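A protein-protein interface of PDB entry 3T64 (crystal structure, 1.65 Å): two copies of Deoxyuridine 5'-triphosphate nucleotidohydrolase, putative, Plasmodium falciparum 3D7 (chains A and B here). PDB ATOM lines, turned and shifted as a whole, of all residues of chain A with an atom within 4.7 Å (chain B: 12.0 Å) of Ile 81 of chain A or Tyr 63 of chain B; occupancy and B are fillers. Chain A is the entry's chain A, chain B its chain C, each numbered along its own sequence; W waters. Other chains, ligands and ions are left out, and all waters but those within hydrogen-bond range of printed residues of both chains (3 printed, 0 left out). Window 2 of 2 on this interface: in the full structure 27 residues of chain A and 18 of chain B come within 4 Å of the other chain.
The backbone carbonyl oxygen of Tyr 63 of chain B is in hydrogen-bond range of the backbone NH of Met 1 of chain A, 2.7 Å away.
SD of Met 1 of chain A lies close to OE1 of Gln 57 of chain A (3.1 Å). The backbone NH of Met 1 of chain A is in hydrogen-bond range of the side-chain carboxylate of Glu 145 of chain A (2.6 Å). O of His 2 of chain A is in hydrogen-bond range of N of Leu 56 of chain A, 2.8 Å away.
Among the printed residues, pairs that only touch across the chains: Tyr 58 of chain A with Tyr 62 of chain B, His 2 of chain A with Lys 65 of chain B, Tyr 58 of chain A with Tyr 63 of chain B, Ile 81 of chain A with Tyr 63 of chain B, Glu 145 of chain A with Tyr 62 of chain B, His 2 of chain A with Tyr 63 of chain B, Leu 56 of chain A with Tyr 63 of chain B and Tyr 58 of chain A with Asn 61 of chain B.
Ile 81 of chain A touches just one residue of chain B: Tyr 63 (3.5 Å). Of chain B, only Tyr 63 (3.6 Å) and Lys 65 (3.4 Å) come within 4 Å of His 2 of chain A. No residue of chain B comes within 4 Å of Gln 57 of chain A. No residue of chain B comes within 4 Å of Lys 59 of chain A. No residue of chain B comes within 4 Å of Val 82 of chain A. No residue of chain B comes within 4 Å of Asn 83 of chain A. Printed residues of chain A within 4 Å of Lys 65 of chain B: His 2 (3.4 Å). Of the printed residues of chain B, Met 1 of chain A touches Tyr 63 (2.7 Å). Of the printed residues of chain B, Glu 145 of chain A touches Tyr 62. The nearest residue of chain B that does not touch Ile 81 of chain A is Lys 65 of chain B (7.4 Å). The nearest printed residue of chain B that does not touch Met 1 of chain A is Tyr 62 of chain B (4.4 Å).
Hydrophobic or aromatic side chains of chain A within 4 Å of the printed part of chain B: His 2, Tyr 58 and Ile 81. Among the printed residues, 9 pairs touch across the chains.
Position printed for both chains: 59. Of the 9 pairs that touch across the chains among the printed residues, none has its exchanged pair printed and touching as well.
Water W2 lies within hydrogen-bond range of the side-chain carboxylate (OE1) of Glu 145 of chain A (2.9 Å), the backbone NH (N) of Tyr 63 of chain B (2.9 Å) and the backbone NH (N) of Tyr 58 of chain A (3.1 Å). Water W1 lies within hydrogen-bond range of the side-chain carboxylate of Glu 145 of chain A (2.9 Å) and the side-chain hydroxyl of Ser 60 of chain B (3.0 Å). Water W3 lies within hydrogen-bond range of N of Tyr 64 of chain B, O of Tyr 62 of chain B and OH of Tyr 58 of chain A.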
ATOM      1  N   MET A   1      24.076  18.223  -5.780  1.00  0.00           N
ATOM      2  CA  MET A   1      25.386  17.541  -5.526  1.00  0.00           C
ATOM      3  C   MET A   1      25.554  16.406  -6.515  1.00  0.00           C
ATOM      4  O   MET A   1      24.607  15.669  -6.776  1.00  0.00           O
ATOM      5  CB  MET A   1      25.439  16.986  -4.097  1.00  0.00           C
ATOM      6  CG  MET A   1      26.817  16.458  -3.702  1.00  0.00           C
ATOM      7  SD  MET A   1      26.926  15.961  -1.973  1.00  0.00           S
ATOM      8  CE  MET A   1      26.239  14.325  -2.061  1.00  0.00           C
ATOM      9  N   HIS A   2      26.758  16.267  -7.059  1.00  0.00           N
ATOM     10  CA  HIS A   2      27.027  15.227  -8.049  1.00  0.00           C
ATOM     11  C   HIS A   2      28.095  14.284  -7.521  1.00  0.00           C
ATOM     12  O   HIS A   2      29.184  14.747  -7.129  1.00  0.00           O
ATOM     13  CB  HIS A   2      27.514  15.868  -9.363  1.00  0.00           C
ATOM     14  CG  HIS A   2      27.780  14.880 -10.453  1.00  0.00           C
ATOM     15  ND1 HIS A   2      26.797  14.058 -10.959  1.00  0.00           N
ATOM     16  CD2 HIS A   2      28.916  14.566 -11.121  1.00  0.00           C
ATOM     17  CE1 HIS A   2      27.315  13.283 -11.900  1.00  0.00           C
ATOM     18  NE2 HIS A   2      28.598  13.580 -12.023  1.00  0.00           N
ATOM     19  N   LEU A  56      30.704  16.465  -5.585  1.00  0.00           N
ATOM     20  CA  LEU A  56      30.993  17.779  -6.179  1.00  0.00           C
ATOM     21  C   LEU A  56      29.826  18.713  -5.966  1.00  0.00           C
ATOM     22  O   LEU A  56      28.683  18.320  -6.174  1.00  0.00           O
ATOM     23  CB  LEU A  56      31.261  17.609  -7.672  1.00  0.00           C
ATOM     24  CG  LEU A  56      32.482  16.775  -8.055  1.00  0.00           C
ATOM     25  CD1 LEU A  56      32.525  16.563  -9.550  1.00  0.00           C
ATOM     26  CD2 LEU A  56      33.731  17.469  -7.586  1.00  0.00           C
ATOM     27  N   GLN A  57      30.130  19.944  -5.542  1.00  0.00           N
ATOM     28  CA  GLN A  57      29.124  20.987  -5.322  1.00  0.00           C
ATOM     29  C   GLN A  57      29.683  22.312  -5.838  1.00  0.00           C
ATOM     30  O   GLN A  57      30.884  22.419  -6.084  1.00  0.00           O
ATOM     31  CB  GLN A  57      28.780  21.119  -3.837  1.00  0.00           C
ATOM     32  CG  GLN A  57      27.953  19.919  -3.337  1.00  0.00           C
ATOM     33  CD  GLN A  57      27.527  19.975  -1.878  1.00  0.00           C
ATOM     34  OE1 GLN A  57      27.030  18.977  -1.349  1.00  0.00           O
ATOM     35  NE2 GLN A  57      27.699  21.121  -1.229  1.00  0.00           N
ATOM     36  N   TYR A  58      28.842  23.304  -6.003  1.00  0.00           N
ATOM     37  CA  TYR A  58      29.318  24.623  -6.379  1.00  0.00           C
ATOM     38  C   TYR A  58      30.083  25.222  -5.196  1.00  0.00           C
ATOM     39  O   TYR A  58      29.668  25.050  -4.100  1.00  0.00           O
ATOM     40  CB  TYR A  58      28.150  25.522  -6.742  1.00  0.00           C
ATOM     41  CG  TYR A  58      27.503  25.261  -8.069  1.00  0.00           C
ATOM     42  CD1 TYR A  58      26.159  25.213  -8.189  1.00  0.00           C
ATOM     43  CD2 TYR A  58      28.239  25.089  -9.184  1.00  0.00           C
ATOM     44  CE1 TYR A  58      25.578  24.978  -9.338  1.00  0.00           C
ATOM     45  CE2 TYR A  58      27.665  24.862 -10.340  1.00  0.00           C
ATOM     46  CZ  TYR A  58      26.335  24.821 -10.427  1.00  0.00           C
ATOM     47  OH  TYR A  58      25.761  24.575 -11.599  1.00  0.00           O
ATOM     48  N   LYS A  59      31.177  25.935  -5.434  1.00  0.00           N
ATOM     49  CA  LYS A  59      31.927  26.624  -4.382  1.00  0.00           C
ATOM     50  C   LYS A  59      31.018  27.635  -3.689  1.00  0.00           C
ATOM     51  O   LYS A  59      30.199  28.196  -4.334  1.00  0.00           O
ATOM     52  CB  LYS A  59      33.115  27.399  -4.963  1.00  0.00           C
ATOM     53  N   ASN A  80      34.995  26.678 -10.163  1.00  0.00           N
ATOM     54  CA  ASN A  80      33.536  26.735 -10.028  1.00  0.00           C
ATOM     55  C   ASN A  80      32.921  25.611  -9.155  1.00  0.00           C
ATOM     56  O   ASN A  80      32.002  25.834  -8.352  1.00  0.00           O
ATOM     57  CB  ASN A  80      32.896  26.658 -11.411  1.00  0.00           C
ATOM     58  CG  ASN A  80      31.426  27.019 -11.386  1.00  0.00           C
ATOM     59  OD1 ASN A  80      31.008  27.904 -10.630  1.00  0.00           O
ATOM     60  ND2 ASN A  80      30.625  26.333 -12.205  1.00  0.00           N
ATOM     61  N   ILE A  81      33.411  24.405  -9.381  1.00  0.00           N
ATOM     62  CA  ILE A  81      32.885  23.188  -8.768  1.00  0.00           C
ATOM     63  C   ILE A  81      34.014  22.663  -7.899  1.00  0.00           C
ATOM     64  O   ILE A  81      35.176  22.693  -8.305  1.00  0.00           O
ATOM     65  CB  ILE A  81      32.500  22.185  -9.882  1.00  0.00           C
ATOM     66  CG1 ILE A  81      31.220  22.660 -10.576  1.00  0.00           C
ATOM     67  CG2 ILE A  81      32.272  20.788  -9.342  1.00  0.00           C
ATOM     68  CD1 ILE A  81      31.133  22.284 -12.062  1.00  0.00           C
ATOM     69  N   VAL A  82      33.688  22.211  -6.689  1.00  0.00           N
ATOM     70  CA  VAL A  82      34.702  21.734  -5.757  1.00  0.00           C
ATOM     71  C   VAL A  82      34.265  20.425  -5.109  1.00  0.00           C
ATOM     72  O   VAL A  82      33.062  20.192  -4.950  1.00  0.00           O
ATOM     73  CB  VAL A  82      35.009  22.759  -4.629  1.00  0.00           C
ATOM     74  CG1 VAL A  82      35.785  23.972  -5.183  1.00  0.00           C
ATOM     75  CG2 VAL A  82      33.724  23.200  -3.911  1.00  0.00           C
ATOM     76  N   ASN A  83      35.254  19.591  -4.783  1.00  0.00           N
ATOM     77  CA  ASN A  83      35.076  18.370  -3.981  1.00  0.00           C
ATOM     78  C   ASN A  83      34.601  18.787  -2.605  1.00  0.00           C
ATOM     79  O   ASN A  83      35.166  19.707  -2.007  1.00  0.00           O
ATOM     80  CB  ASN A  83      36.422  17.648  -3.785  1.00  0.00           C
ATOM     81  CG  ASN A  83      36.819  16.799  -4.960  1.00  0.00           C
ATOM     82  OD1 ASN A  83      37.885  16.166  -4.945  1.00  0.00           O
ATOM     83  ND2 ASN A  83      35.976  16.755  -5.982  1.00  0.00           N
ATOM     84  N   GLU A 145      20.319  18.816  -0.953  1.00  0.00           N
ATOM     85  CA  GLU A 145      19.963  19.066  -2.354  1.00  0.00           C
ATOM     86  C   GLU A 145      19.866  17.755  -3.139  1.00  0.00           C
ATOM     87  O   GLU A 145      20.466  16.740  -2.744  1.00  0.00           O
ATOM     88  CB  GLU A 145      21.002  19.995  -3.022  1.00  0.00           C
ATOM     89  CG  GLU A 145      22.446  19.440  -3.059  1.00  0.00           C
ATOM     90  CD  GLU A 145      23.500  20.506  -3.350  1.00  0.00           C
ATOM     91  OE1 GLU A 145      24.351  20.295  -4.235  1.00  0.00           O
ATOM     92  OE2 GLU A 145      23.495  21.569  -2.690  1.00  0.00           O
ATOM     93  N   LYS B  59      14.732  29.059  -3.205  1.00  0.00           N
ATOM     94  CA  LYS B  59      15.454  28.279  -4.188  1.00  0.00           C
ATOM     95  C   LYS B  59      16.916  28.673  -4.167  1.00  0.00           C
ATOM     96  O   LYS B  59      17.254  29.847  -4.060  1.00  0.00           O
ATOM     97  CB  LYS B  59      14.877  28.498  -5.588  1.00  0.00           C
ATOM     98  N   SER B  60      17.776  27.665  -4.219  1.00  0.00           N
ATOM     99  CA  SER B  60      19.206  27.883  -4.336  1.00  0.00           C
ATOM    100  C   SER B  60      19.702  27.094  -5.539  1.00  0.00           C
ATOM    101  O   SER B  60      19.093  26.087  -5.931  1.00  0.00           O
ATOM    102  CB  SER B  60      19.927  27.436  -3.062  1.00  0.00           C
ATOM    103  OG  SER B  60      19.705  26.062  -2.814  1.00  0.00           O
ATOM    104  N   ASN B  61      20.776  27.565  -6.158  1.00  0.00           N
ATOM    105  CA  ASN B  61      21.383  26.837  -7.268  1.00  0.00           C
ATOM    106  C   ASN B  61      22.279  25.722  -6.752  1.00  0.00           C
ATOM    107  O   ASN B  61      23.092  25.938  -5.856  1.00  0.00           O
ATOM    108  CB  ASN B  61      22.132  27.756  -8.257  1.00  0.00           C
ATOM    109  CG  ASN B  61      22.913  28.881  -7.575  1.00  0.00           C
ATOM    110  OD1 ASN B  61      22.870  30.034  -8.020  1.00  0.00           O
ATOM    111  ND2 ASN B  61      23.636  28.553  -6.507  1.00  0.00           N
ATOM    112  N   TYR B  62      22.114  24.531  -7.312  1.00  0.00           N
ATOM    113  CA  TYR B  62      22.925  23.387  -6.898  1.00  0.00           C
ATOM    114  C   TYR B  62      23.495  22.663  -8.111  1.00  0.00           C
ATOM    115  O   TYR B  62      22.888  22.662  -9.190  1.00  0.00           O
ATOM    116  CB  TYR B  62      22.097  22.425  -6.037  1.00  0.00           C
ATOM    117  CG  TYR B  62      20.832  21.916  -6.704  1.00  0.00           C
ATOM    118  CD1 TYR B  62      19.619  22.595  -6.562  1.00  0.00           C
ATOM    119  CD2 TYR B  62      20.846  20.752  -7.469  1.00  0.00           C
ATOM    120  CE1 TYR B  62      18.461  22.125  -7.179  1.00  0.00           C
ATOM    121  CE2 TYR B  62      19.713  20.283  -8.080  1.00  0.00           C
ATOM    122  CZ  TYR B  62      18.521  20.968  -7.938  1.00  0.00           C
ATOM    123  OH  TYR B  62      17.395  20.476  -8.555  1.00  0.00           O
ATOM    124  N   TYR B  63      24.655  22.044  -7.921  1.00  0.00           N
ATOM    125  CA  TYR B  63      25.312  21.300  -8.996  1.00  0.00           C
ATOM    126  C   TYR B  63      24.709  19.903  -9.170  1.00  0.00           C
ATOM    127  O   TYR B  63      24.692  19.109  -8.236  1.00  0.00           O
ATOM    128  CB  TYR B  63      26.819  21.231  -8.762  1.00  0.00           C
ATOM    129  CG  TYR B  63      27.555  20.590  -9.906  1.00  0.00           C
ATOM    130  CD1 TYR B  63      27.477  21.123 -11.199  1.00  0.00           C
ATOM    131  CD2 TYR B  63      28.338  19.465  -9.708  1.00  0.00           C
ATOM    132  CE1 TYR B  63      28.152  20.537 -12.251  1.00  0.00           C
ATOM    133  CE2 TYR B  63      29.025  18.877 -10.755  1.00  0.00           C
ATOM    134  CZ  TYR B  63      28.925  19.418 -12.023  1.00  0.00           C
ATOM    135  OH  TYR B  63      29.601  18.822 -13.056  1.00  0.00           O
ATOM    136  N   TYR B  64      24.225  19.621 -10.378  1.00  0.00           N
ATOM    137  CA  TYR B  64      23.497  18.394 -10.674  1.00  0.00           C
ATOM    138  C   TYR B  64      23.715  18.070 -12.147  1.00  0.00           C
ATOM    139  O   TYR B  64      23.677  18.982 -12.996  1.00  0.00           O
ATOM    140  CB  TYR B  64      21.998  18.597 -10.363  1.00  0.00           C
ATOM    141  CG  TYR B  64      21.103  17.399 -10.587  1.00  0.00           C
ATOM    142  CD1 TYR B  64      20.661  16.621  -9.507  1.00  0.00           C
ATOM    143  CD2 TYR B  64      20.676  17.051 -11.874  1.00  0.00           C
ATOM    144  CE1 TYR B  64      19.826  15.514  -9.705  1.00  0.00           C
ATOM    145  CE2 TYR B  64      19.852  15.951 -12.084  1.00  0.00           C
ATOM    146  CZ  TYR B  64      19.426  15.189 -11.000  1.00  0.00           C
ATOM    147  OH  TYR B  64      18.613  14.099 -11.223  1.00  0.00           O
ATOM    148  N   LYS B  65      23.945  16.796 -12.460  1.00  0.00           N
ATOM    149  CA  LYS B  65      24.158  16.371 -13.853  1.00  0.00           C
ATOM    150  C   LYS B  65      23.027  15.520 -14.422  1.00  0.00           C
ATOM    151  O   LYS B  65      22.443  14.687 -13.729  1.00  0.00           O
ATOM    152  CB  LYS B  65      25.489  15.643 -14.004  1.00  0.00           C
ATOM    153  CG  LYS B  65      26.681  16.563 -13.958  1.00  0.00           C
ATOM    154  CD  LYS B  65      27.950  15.858 -14.405  1.00  0.00           C
ATOM    155  CE  LYS B  65      28.029  15.723 -15.913  1.00  0.00           C
ATOM    156  NZ  LYS B  65      28.528  16.970 -16.541  1.00  0.00           N
HETATM  157  O   HOH W   1      21.671  23.809  -2.780  1.00  0.00           O
HETATM  158  O   HOH W   2      25.984  22.359  -5.377  1.00  0.00           O
HETATM  159  O   HOH W   3      23.671  22.123 -12.203  1.00  0.00           O
